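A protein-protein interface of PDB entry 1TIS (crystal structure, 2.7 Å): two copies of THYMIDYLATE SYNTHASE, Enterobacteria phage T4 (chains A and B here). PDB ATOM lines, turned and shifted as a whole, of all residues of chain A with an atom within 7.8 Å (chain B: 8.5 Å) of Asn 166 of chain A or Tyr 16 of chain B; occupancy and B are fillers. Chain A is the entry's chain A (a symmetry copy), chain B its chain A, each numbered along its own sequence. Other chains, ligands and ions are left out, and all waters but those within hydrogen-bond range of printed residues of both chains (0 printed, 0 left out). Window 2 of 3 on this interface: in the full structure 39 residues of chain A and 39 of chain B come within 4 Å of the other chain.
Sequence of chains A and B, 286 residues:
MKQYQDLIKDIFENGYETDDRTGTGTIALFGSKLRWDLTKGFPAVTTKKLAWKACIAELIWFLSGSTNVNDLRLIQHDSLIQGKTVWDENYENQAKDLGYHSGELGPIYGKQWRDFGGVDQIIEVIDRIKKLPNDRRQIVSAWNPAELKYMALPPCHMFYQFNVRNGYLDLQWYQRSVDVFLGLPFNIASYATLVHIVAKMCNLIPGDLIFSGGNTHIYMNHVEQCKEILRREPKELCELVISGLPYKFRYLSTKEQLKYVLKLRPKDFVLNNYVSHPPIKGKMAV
Hydrophobic or aromatic side chains of chain B within 4 Å of the printed part of chain A: Tyr 16 and Phe 30.
Among the printed residues, no Asp or Glu carboxylate lies within 4 Å of a Lys or Arg side-chain nitrogen of the other chain.
No position is printed for both chains.
OH of Tyr 16 of chain B is in hydrogen-bond range of N of Asn 166 of chain A.
The backbone carbonyl oxygen (O) of Asp 19 of chain B lies within hydrogen-bond range of the side-chain amide nitrogen (ND2) of Asn 134 of chain A.
OD1 of Asn 163 of chain A lies close to OD1 of Asn 215 of chain B (3.4 Å).
N of Tyr 16 of chain B sits at hydrogen-bond distance from OD1 of Asn 14 of chain B (2.5 Å).
The backbone carbonyl oxygen of Tyr 16 of chain B is in hydrogen-bond range of the backbone NH of Ala 28 of chain B (3.3 Å).
O of Thr 26 of chain B lies within hydrogen-bond range of N of Thr 18 of chain B, 2.8 Å away.
OD1 of Asp 20 of chain B lies within hydrogen-bond range of OG1 of Thr 26 of chain B, 3.5 Å away.
ND2 of Asn 134 of chain A lies within hydrogen-bond range of O of Val 164 of chain A, at 3.5 Å.
N of Asp 170 of chain A is in hydrogen-bond range of O of Asn 163 of chain A.
Among the printed residues, merely in contact across the chains: Asn 163 of chain A with Phe 30 of chain B, Arg 165 of chain A with Tyr 16 of chain B, Asn 134 of chain A with Asp 20 of chain B, Asn 134 of chain A with Thr 18 of chain B and Asp 170 of chain A with Phe 30 of chain B.
Of the printed residues of chain B, Asn 163 of chain A touches Phe 30 (3.0 Å) and Asn 215 (3.4 Å).
Val 164 of chain A touches none of the printed residues of chain B.
Printed residues of chain B within 4 Å of Arg 165 of chain A: Tyr 16 (3.6 Å).
Of the printed residues of chain B, Asn 166 of chain A touches Tyr 16 (2.9 Å).
Of chain A, only Arg 165 (3.6 Å) and Asn 166 (2.9 Å) come within 4 Å of Tyr 16 of chain B.
Printed residues of chain A within 4 Å of Thr 18 of chain B: Asn 134 (3.7 Å).
Printed residues of chain A within 4 Å of Asp 20 of chain B: Asn 134.
Of the printed residues of chain A, Phe 30 of chain B touches Asn 163 and Asp 170.
The nearest residue of chain A that does not touch Tyr 16 of chain B is Tyr 168 of chain A (4.3 Å).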
ATOM      1  N   ASN A 134      13.377   1.166 -24.481  1.00  0.00           N
ATOM      2  CA  ASN A 134      12.516   0.967 -23.338  1.00  0.00           C
ATOM      3  C   ASN A 134      12.419  -0.517 -22.921  1.00  0.00           C
ATOM      4  O   ASN A 134      11.391  -0.988 -22.410  1.00  0.00           O
ATOM      5  CB  ASN A 134      11.127   1.621 -23.672  1.00  0.00           C
ATOM      6  CG  ASN A 134      10.998   3.131 -23.311  1.00  0.00           C
ATOM      7  OD1 ASN A 134      11.075   4.056 -24.135  1.00  0.00           O
ATOM      8  ND2 ASN A 134      10.762   3.465 -22.053  1.00  0.00           N
ATOM      9  N   ASN A 163      18.059   2.758 -17.539  1.00  0.00           N
ATOM     10  CA  ASN A 163      16.644   3.014 -17.838  1.00  0.00           C
ATOM     11  C   ASN A 163      16.664   4.129 -18.862  1.00  0.00           C
ATOM     12  O   ASN A 163      17.500   5.036 -18.747  1.00  0.00           O
ATOM     13  CB  ASN A 163      15.900   3.527 -16.628  1.00  0.00           C
ATOM     14  CG  ASN A 163      14.518   2.945 -16.437  1.00  0.00           C
ATOM     15  OD1 ASN A 163      14.362   1.809 -15.998  1.00  0.00           O
ATOM     16  ND2 ASN A 163      13.453   3.697 -16.658  1.00  0.00           N
ATOM     17  N   VAL A 164      15.826   4.101 -19.885  1.00  0.00           N
ATOM     18  CA  VAL A 164      15.758   5.179 -20.874  1.00  0.00           C
ATOM     19  C   VAL A 164      14.446   5.977 -20.657  1.00  0.00           C
ATOM     20  O   VAL A 164      13.361   5.374 -20.736  1.00  0.00           O
ATOM     21  CB  VAL A 164      15.832   4.522 -22.277  1.00  0.00           C
ATOM     22  CG1 VAL A 164      15.876   5.615 -23.325  1.00  0.00           C
ATOM     23  CG2 VAL A 164      17.056   3.623 -22.391  1.00  0.00           C
ATOM     24  N   ARG A 165      14.533   7.284 -20.270  1.00  0.00           N
ATOM     25  CA  ARG A 165      13.374   8.165 -20.028  1.00  0.00           C
ATOM     26  C   ARG A 165      12.642   8.533 -21.320  1.00  0.00           C
ATOM     27  O   ARG A 165      12.009   7.675 -21.933  1.00  0.00           O
ATOM     28  CB  ARG A 165      13.828   9.438 -19.313  1.00  0.00           C
ATOM     29  CG  ARG A 165      13.872   9.104 -17.838  1.00  0.00           C
ATOM     30  CD  ARG A 165      13.659  10.251 -16.855  1.00  0.00           C
ATOM     31  NE  ARG A 165      14.553  11.383 -17.078  1.00  0.00           N
ATOM     32  CZ  ARG A 165      14.700  12.388 -16.203  1.00  0.00           C
ATOM     33  NH1 ARG A 165      14.017  12.393 -15.062  1.00  0.00           N
ATOM     34  NH2 ARG A 165      15.535  13.409 -16.455  1.00  0.00           N
ATOM     35  N   ASN A 166      12.533   9.773 -21.774  1.00  0.00           N
ATOM     36  CA  ASN A 166      12.133   9.959 -23.152  1.00  0.00           C
ATOM     37  C   ASN A 166      13.208  10.979 -23.365  1.00  0.00           C
ATOM     38  O   ASN A 166      13.040  12.175 -23.106  1.00  0.00           O
ATOM     39  CB  ASN A 166      10.746  10.616 -23.383  1.00  0.00           C
ATOM     40  CG  ASN A 166       9.931  10.161 -24.613  1.00  0.00           C
ATOM     41  OD1 ASN A 166       8.729  10.429 -24.681  1.00  0.00           O
ATOM     42  ND2 ASN A 166      10.399   9.438 -25.630  1.00  0.00           N
ATOM     43  N   GLY A 167      14.380  10.393 -23.651  1.00  0.00           N
ATOM     44  CA  GLY A 167      15.523  11.222 -23.973  1.00  0.00           C
ATOM     45  C   GLY A 167      16.571  11.324 -22.887  1.00  0.00           C
ATOM     46  O   GLY A 167      17.546  12.065 -23.009  1.00  0.00           O
ATOM     47  N   TYR A 168      16.398  10.603 -21.792  1.00  0.00           N
ATOM     48  CA  TYR A 168      17.449  10.569 -20.797  1.00  0.00           C
ATOM     49  C   TYR A 168      17.842   9.102 -20.549  1.00  0.00           C
ATOM     50  O   TYR A 168      17.123   8.139 -20.877  1.00  0.00           O
ATOM     51  CB  TYR A 168      16.964  11.242 -19.525  1.00  0.00           C
ATOM     52  CG  TYR A 168      16.549  12.701 -19.671  1.00  0.00           C
ATOM     53  CD1 TYR A 168      15.239  12.986 -20.010  1.00  0.00           C
ATOM     54  CD2 TYR A 168      17.409  13.745 -19.368  1.00  0.00           C
ATOM     55  CE1 TYR A 168      14.768  14.287 -20.030  1.00  0.00           C
ATOM     56  CE2 TYR A 168      16.940  15.051 -19.380  1.00  0.00           C
ATOM     57  CZ  TYR A 168      15.614  15.323 -19.707  1.00  0.00           C
ATOM     58  OH  TYR A 168      15.086  16.619 -19.649  1.00  0.00           O
ATOM     59  N   LEU A 169      19.064   8.958 -20.076  1.00  0.00           N
ATOM     60  CA  LEU A 169      19.629   7.666 -19.771  1.00  0.00           C
ATOM     61  C   LEU A 169      19.781   7.682 -18.282  1.00  0.00           C
ATOM     62  O   LEU A 169      20.184   8.704 -17.725  1.00  0.00           O
ATOM     63  CB  LEU A 169      20.985   7.517 -20.394  1.00  0.00           C
ATOM     64  CG  LEU A 169      21.746   6.261 -20.139  1.00  0.00           C
ATOM     65  CD1 LEU A 169      21.000   5.063 -20.714  1.00  0.00           C
ATOM     66  CD2 LEU A 169      23.108   6.432 -20.747  1.00  0.00           C
ATOM     67  N   ASP A 170      19.487   6.611 -17.592  1.00  0.00           N
ATOM     68  CA  ASP A 170      19.620   6.651 -16.158  1.00  0.00           C
ATOM     69  C   ASP A 170      20.479   5.461 -15.770  1.00  0.00           C
ATOM     70  O   ASP A 170      20.362   4.449 -16.478  1.00  0.00           O
ATOM     71  CB  ASP A 170      18.235   6.554 -15.523  1.00  0.00           C
ATOM     72  CG  ASP A 170      17.175   7.568 -15.970  1.00  0.00           C
ATOM     73  OD1 ASP A 170      17.481   8.734 -16.227  1.00  0.00           O
ATOM     74  OD2 ASP A 170      16.013   7.173 -16.039  1.00  0.00           O
ATOM     75  N   LEU A 204      21.854  10.297 -26.058  1.00  0.00           N
ATOM     76  CA  LEU A 204      20.788  10.553 -25.163  1.00  0.00           C
ATOM     77  C   LEU A 204      21.368  11.597 -24.226  1.00  0.00           C
ATOM     78  O   LEU A 204      22.578  11.846 -24.146  1.00  0.00           O
ATOM     79  CB  LEU A 204      20.412   9.236 -24.471  1.00  0.00           C
ATOM     80  CG  LEU A 204      19.994   7.956 -25.248  1.00  0.00           C
ATOM     81  CD1 LEU A 204      19.115   7.083 -24.392  1.00  0.00           C
ATOM     82  CD2 LEU A 204      19.094   8.269 -26.396  1.00  0.00           C
ATOM     83  N   ILE A 205      20.447  12.254 -23.543  1.00  0.00           N
ATOM     84  CA  ILE A 205      20.772  13.295 -22.581  1.00  0.00           C
ATOM     85  C   ILE A 205      21.022  12.477 -21.335  1.00  0.00           C
ATOM     86  O   ILE A 205      20.172  11.683 -20.923  1.00  0.00           O
ATOM     87  CB  ILE A 205      19.571  14.284 -22.328  1.00  0.00           C
ATOM     88  CG1 ILE A 205      19.019  14.924 -23.634  1.00  0.00           C
ATOM     89  CG2 ILE A 205      20.053  15.321 -21.331  1.00  0.00           C
ATOM     90  CD1 ILE A 205      19.978  15.639 -24.625  1.00  0.00           C
ATOM     91  N   ILE B  11       4.454   7.080  -7.407  1.00  0.00           N
ATOM     92  CA  ILE B  11       4.642   6.684  -8.801  1.00  0.00           C
ATOM     93  C   ILE B  11       3.755   7.636  -9.596  1.00  0.00           C
ATOM     94  O   ILE B  11       4.230   8.118 -10.613  1.00  0.00           O
ATOM     95  CB  ILE B  11       4.178   5.247  -9.089  1.00  0.00           C
ATOM     96  CG1 ILE B  11       4.982   4.283  -8.289  1.00  0.00           C
ATOM     97  CG2 ILE B  11       4.371   4.913 -10.544  1.00  0.00           C
ATOM     98  CD1 ILE B  11       4.159   3.023  -8.022  1.00  0.00           C
ATOM     99  N   PHE B  12       2.515   7.997  -9.201  1.00  0.00           N
ATOM    100  CA  PHE B  12       1.649   8.940  -9.941  1.00  0.00           C
ATOM    101  C   PHE B  12       2.380  10.222 -10.384  1.00  0.00           C
ATOM    102  O   PHE B  12       2.532  10.512 -11.586  1.00  0.00           O
ATOM    103  CB  PHE B  12       0.446   9.418  -9.113  1.00  0.00           C
ATOM    104  CG  PHE B  12      -0.485   8.412  -8.451  1.00  0.00           C
ATOM    105  CD1 PHE B  12      -0.377   7.049  -8.657  1.00  0.00           C
ATOM    106  CD2 PHE B  12      -1.460   8.917  -7.604  1.00  0.00           C
ATOM    107  CE1 PHE B  12      -1.250   6.204  -8.007  1.00  0.00           C
ATOM    108  CE2 PHE B  12      -2.331   8.070  -6.957  1.00  0.00           C
ATOM    109  CZ  PHE B  12      -2.224   6.712  -7.162  1.00  0.00           C
ATOM    110  N   GLU B  13       2.934  10.967  -9.420  1.00  0.00           N
ATOM    111  CA  GLU B  13       3.651  12.183  -9.755  1.00  0.00           C
ATOM    112  C   GLU B  13       4.958  11.949 -10.528  1.00  0.00           C
ATOM    113  O   GLU B  13       5.526  12.937 -11.003  1.00  0.00           O
ATOM    114  CB  GLU B  13       3.927  12.970  -8.460  1.00  0.00           C
ATOM    115  CG  GLU B  13       5.034  12.499  -7.487  1.00  0.00           C
ATOM    116  CD  GLU B  13       6.505  12.783  -7.834  1.00  0.00           C
ATOM    117  OE1 GLU B  13       6.795  13.706  -8.600  1.00  0.00           O
ATOM    118  OE2 GLU B  13       7.366  12.068  -7.321  1.00  0.00           O
ATOM    119  N   ASN B  14       5.461  10.704 -10.657  1.00  0.00           N
ATOM    120  CA  ASN B  14       6.682  10.337 -11.385  1.00  0.00           C
ATOM    121  C   ASN B  14       7.041  11.047 -12.678  1.00  0.00           C
ATOM    122  O   ASN B  14       8.211  11.094 -13.050  1.00  0.00           O
ATOM    123  CB  ASN B  14       6.694   8.886 -11.792  1.00  0.00           C
ATOM    124  CG  ASN B  14       5.899   8.663 -13.077  1.00  0.00           C
ATOM    125  OD1 ASN B  14       6.459   8.474 -14.136  1.00  0.00           O
ATOM    126  ND2 ASN B  14       4.611   8.884 -13.199  1.00  0.00           N
ATOM    127  N   GLY B  15       5.996  11.402 -13.433  1.00  0.00           N
ATOM    128  CA  GLY B  15       6.117  12.060 -14.717  1.00  0.00           C
ATOM    129  C   GLY B  15       5.882  11.128 -15.906  1.00  0.00           C
ATOM    130  O   GLY B  15       4.999  11.381 -16.737  1.00  0.00           O
ATOM    131  N   TYR B  16       6.665  10.051 -16.002  1.00  0.00           N
ATOM    132  CA  TYR B  16       6.642   9.152 -17.141  1.00  0.00           C
ATOM    133  C   TYR B  16       5.567   8.075 -17.305  1.00  0.00           C
ATOM    134  O   TYR B  16       5.597   6.905 -16.898  1.00  0.00           O
ATOM    135  CB  TYR B  16       8.075   8.557 -17.231  1.00  0.00           C
ATOM    136  CG  TYR B  16       8.933   9.475 -18.121  1.00  0.00           C
ATOM    137  CD1 TYR B  16       8.871   9.338 -19.501  1.00  0.00           C
ATOM    138  CD2 TYR B  16       9.724  10.481 -17.576  1.00  0.00           C
ATOM    139  CE1 TYR B  16       9.571  10.186 -20.322  1.00  0.00           C
ATOM    140  CE2 TYR B  16      10.436  11.337 -18.400  1.00  0.00           C
ATOM    141  CZ  TYR B  16      10.350  11.176 -19.767  1.00  0.00           C
ATOM    142  OH  TYR B  16      11.098  11.989 -20.589  1.00  0.00           O
ATOM    143  N   GLU B  17       4.551   8.608 -17.979  1.00  0.00           N
ATOM    144  CA  GLU B  17       3.398   7.862 -18.463  1.00  0.00           C
ATOM    145  C   GLU B  17       3.968   7.420 -19.789  1.00  0.00           C
ATOM    146  O   GLU B  17       3.937   8.139 -20.789  1.00  0.00           O
ATOM    147  CB  GLU B  17       2.144   8.788 -18.646  1.00  0.00           C
ATOM    148  CG  GLU B  17       2.368  10.237 -19.159  1.00  0.00           C
ATOM    149  CD  GLU B  17       1.198  10.950 -19.837  1.00  0.00           C
ATOM    150  OE1 GLU B  17       0.178  10.312 -20.108  1.00  0.00           O
ATOM    151  OE2 GLU B  17       1.319  12.150 -20.105  1.00  0.00           O
ATOM    152  N   THR B  18       4.556   6.255 -19.838  1.00  0.00           N
ATOM    153  CA  THR B  18       5.297   5.968 -21.034  1.00  0.00           C
ATOM    154  C   THR B  18       5.135   4.595 -21.684  1.00  0.00           C
ATOM    155  O   THR B  18       4.593   3.612 -21.155  1.00  0.00           O
ATOM    156  CB  THR B  18       6.742   6.408 -20.560  1.00  0.00           C
ATOM    157  OG1 THR B  18       6.672   7.832 -20.731  1.00  0.00           O
ATOM    158  CG2 THR B  18       7.974   5.831 -21.262  1.00  0.00           C
ATOM    159  N   ASP B  19       5.495   4.675 -22.967  1.00  0.00           N
ATOM    160  CA  ASP B  19       5.614   3.536 -23.860  1.00  0.00           C
ATOM    161  C   ASP B  19       6.788   2.697 -23.323  1.00  0.00           C
ATOM    162  O   ASP B  19       7.650   3.141 -22.552  1.00  0.00           O
ATOM    163  CB  ASP B  19       5.863   4.048 -25.295  1.00  0.00           C
ATOM    164  CG  ASP B  19       5.046   3.295 -26.336  1.00  0.00           C
ATOM    165  OD1 ASP B  19       3.814   3.254 -26.236  1.00  0.00           O
ATOM    166  OD2 ASP B  19       5.656   2.743 -27.246  1.00  0.00           O
ATOM    167  N   ASP B  20       6.865   1.463 -23.768  1.00  0.00           N
ATOM    168  CA  ASP B  20       7.653   0.471 -23.067  1.00  0.00           C
ATOM    169  C   ASP B  20       7.919  -0.648 -24.080  1.00  0.00           C
ATOM    170  O   ASP B  20       7.871  -0.365 -25.281  1.00  0.00           O
ATOM    171  CB  ASP B  20       6.778   0.061 -21.841  1.00  0.00           C
ATOM    172  CG  ASP B  20       5.290  -0.194 -22.170  1.00  0.00           C
ATOM    173  OD1 ASP B  20       4.493   0.743 -22.280  1.00  0.00           O
ATOM    174  OD2 ASP B  20       4.923  -1.352 -22.343  1.00  0.00           O
ATOM    175  N   GLY B  25       0.540   1.559 -22.432  1.00  0.00           N
ATOM    176  CA  GLY B  25       1.081   2.642 -21.641  1.00  0.00           C
ATOM    177  C   GLY B  25       1.214   2.149 -20.196  1.00  0.00           C
ATOM    178  O   GLY B  25       0.522   1.206 -19.774  1.00  0.00           O
ATOM    179  N   THR B  26       2.038   2.826 -19.403  1.00  0.00           N
ATOM    180  CA  THR B  26       2.304   2.471 -18.020  1.00  0.00           C
ATOM    181  C   THR B  26       2.611   3.810 -17.344  1.00  0.00           C
ATOM    182  O   THR B  26       2.985   4.767 -18.041  1.00  0.00           O
ATOM    183  CB  THR B  26       3.547   1.543 -17.964  1.00  0.00           C
ATOM    184  OG1 THR B  26       3.415   0.555 -18.967  1.00  0.00           O
ATOM    185  CG2 THR B  26       3.659   0.763 -16.685  1.00  0.00           C
ATOM    186  N   ILE B  27       2.415   3.970 -16.037  1.00  0.00           N
ATOM    187  CA  ILE B  27       2.944   5.122 -15.289  1.00  0.00           C
ATOM    188  C   ILE B  27       4.016   4.375 -14.479  1.00  0.00           C
ATOM    189  O   ILE B  27       3.695   3.297 -13.933  1.00  0.00           O
ATOM    190  CB  ILE B  27       1.808   5.733 -14.419  1.00  0.00           C
ATOM    191  CG1 ILE B  27       1.292   6.946 -15.173  1.00  0.00           C
ATOM    192  CG2 ILE B  27       2.262   6.129 -13.006  1.00  0.00           C
ATOM    193  CD1 ILE B  27       2.181   8.220 -15.135  1.00  0.00           C
ATOM    194  N   ALA B  28       5.276   4.814 -14.377  1.00  0.00           N
ATOM    195  CA  ALA B  28       6.297   3.989 -13.762  1.00  0.00           C
ATOM    196  C   ALA B  28       7.399   4.853 -13.231  1.00  0.00           C
ATOM    197  O   ALA B  28       7.538   5.949 -13.742  1.00  0.00           O
ATOM    198  CB  ALA B  28       6.893   3.062 -14.780  1.00  0.00           C
ATOM    199  N   LEU B  29       8.242   4.449 -12.281  1.00  0.00           N
ATOM    200  CA  LEU B  29       9.272   5.300 -11.705  1.00  0.00           C
ATOM    201  C   LEU B  29      10.429   4.326 -11.549  1.00  0.00           C
ATOM    202  O   LEU B  29      10.266   3.204 -11.052  1.00  0.00           O
ATOM    203  CB  LEU B  29       8.729   5.835 -10.343  1.00  0.00           C
ATOM    204  CG  LEU B  29       9.436   6.742  -9.292  1.00  0.00           C
ATOM    205  CD1 LEU B  29       9.459   8.219  -9.657  1.00  0.00           C
ATOM    206  CD2 LEU B  29       8.621   6.656  -8.020  1.00  0.00           C
ATOM    207  N   PHE B  30      11.618   4.720 -11.994  1.00  0.00           N
ATOM    208  CA  PHE B  30      12.834   3.891 -11.865  1.00  0.00           C
ATOM    209  C   PHE B  30      13.636   4.220 -10.608  1.00  0.00           C
ATOM    210  O   PHE B  30      14.150   5.334 -10.465  1.00  0.00           O
ATOM    211  CB  PHE B  30      13.739   4.098 -13.113  1.00  0.00           C
ATOM    212  CG  PHE B  30      15.121   3.452 -13.098  1.00  0.00           C
ATOM    213  CD1 PHE B  30      15.252   2.073 -13.173  1.00  0.00           C
ATOM    214  CD2 PHE B  30      16.251   4.270 -13.020  1.00  0.00           C
ATOM    215  CE1 PHE B  30      16.513   1.521 -13.164  1.00  0.00           C
ATOM    216  CE2 PHE B  30      17.510   3.707 -13.014  1.00  0.00           C
ATOM    217  CZ  PHE B  30      17.631   2.332 -13.087  1.00  0.00           C
ATOM    218  N   ASN B 215      12.680  -0.842 -12.596  1.00  0.00           N
ATOM    219  CA  ASN B 215      11.490  -0.241 -13.151  1.00  0.00           C
ATOM    220  C   ASN B 215      10.208  -0.700 -12.479  1.00  0.00           C
ATOM    221  O   ASN B 215       9.551  -1.675 -12.889  1.00  0.00           O
ATOM    222  CB  ASN B 215      11.442  -0.556 -14.595  1.00  0.00           C
ATOM    223  CG  ASN B 215      10.535   0.385 -15.333  1.00  0.00           C
ATOM    224  OD1 ASN B 215      10.986   1.196 -16.133  1.00  0.00           O
ATOM    225  ND2 ASN B 215       9.232   0.315 -15.124  1.00  0.00           N
ATOM    226  N   THR B 216       9.874   0.051 -11.438  1.00  0.00           N
ATOM    227  CA  THR B 216       8.613  -0.042 -10.688  1.00  0.00           C
ATOM    228  C   THR B 216       7.516   0.608 -11.552  1.00  0.00           C
ATOM    229  O   THR B 216       7.509   1.788 -11.923  1.00  0.00           O
ATOM    230  CB  THR B 216       8.791   0.693  -9.339  1.00  0.00           C
ATOM    231  OG1 THR B 216       9.724  -0.069  -8.571  1.00  0.00           O
ATOM    232  CG2 THR B 216       7.508   0.836  -8.567  1.00  0.00           C
ATOM    233  N   HIS B 217       6.549  -0.204 -11.919  1.00  0.00           N
ATOM    234  CA  HIS B 217       5.561   0.259 -12.830  1.00  0.00           C
ATOM    235  C   HIS B 217       4.174  -0.237 -12.449  1.00  0.00           C
ATOM    236  O   HIS B 217       4.031  -1.302 -11.820  1.00  0.00           O
ATOM    237  CB  HIS B 217       6.042  -0.212 -14.195  1.00  0.00           C
ATOM    238  CG  HIS B 217       6.195  -1.707 -14.508  1.00  0.00           C
ATOM    239  ND1 HIS B 217       5.423  -2.774 -14.276  1.00  0.00           N
ATOM    240  CD2 HIS B 217       7.271  -2.176 -15.218  1.00  0.00           C
ATOM    241  CE1 HIS B 217       5.970  -3.836 -14.814  1.00  0.00           C
ATOM    242  NE2 HIS B 217       7.085  -3.451 -15.373  1.00  0.00           N
ATOM    243  N   ILE B 218       3.164   0.535 -12.842  1.00  0.00           N
ATOM    244  CA  ILE B 218       1.759   0.230 -12.661  1.00  0.00           C
ATOM    245  C   ILE B 218       1.248   0.246 -14.095  1.00  0.00           C
ATOM    246  O   ILE B 218       1.556   1.208 -14.807  1.00  0.00           O
ATOM    247  CB  ILE B 218       1.090   1.336 -11.868  1.00  0.00           C
ATOM    248  CG1 ILE B 218       1.713   1.545 -10.503  1.00  0.00           C
ATOM    249  CG2 ILE B 218      -0.371   0.949 -11.756  1.00  0.00           C
ATOM    250  CD1 ILE B 218       1.059   2.740  -9.801  1.00  0.00           C
ATOM    251  N   MET B 220      -1.331   0.723 -17.373  1.00  0.00           N
ATOM    252  CA  MET B 220      -2.462   1.620 -17.585  1.00  0.00           C
ATOM    253  C   MET B 220      -3.854   0.957 -17.707  1.00  0.00           C
ATOM    254  O   MET B 220      -4.802   1.500 -18.290  1.00  0.00           O
ATOM    255  CB  MET B 220      -2.136   2.468 -18.821  1.00  0.00           C
ATOM    256  CG  MET B 220      -1.321   3.737 -18.460  1.00  0.00           C
ATOM    257  SD  MET B 220      -0.468   4.649 -19.805  1.00  0.00           S
ATOM    258  CE  MET B 220      -1.753   5.101 -20.945  1.00  0.00           C
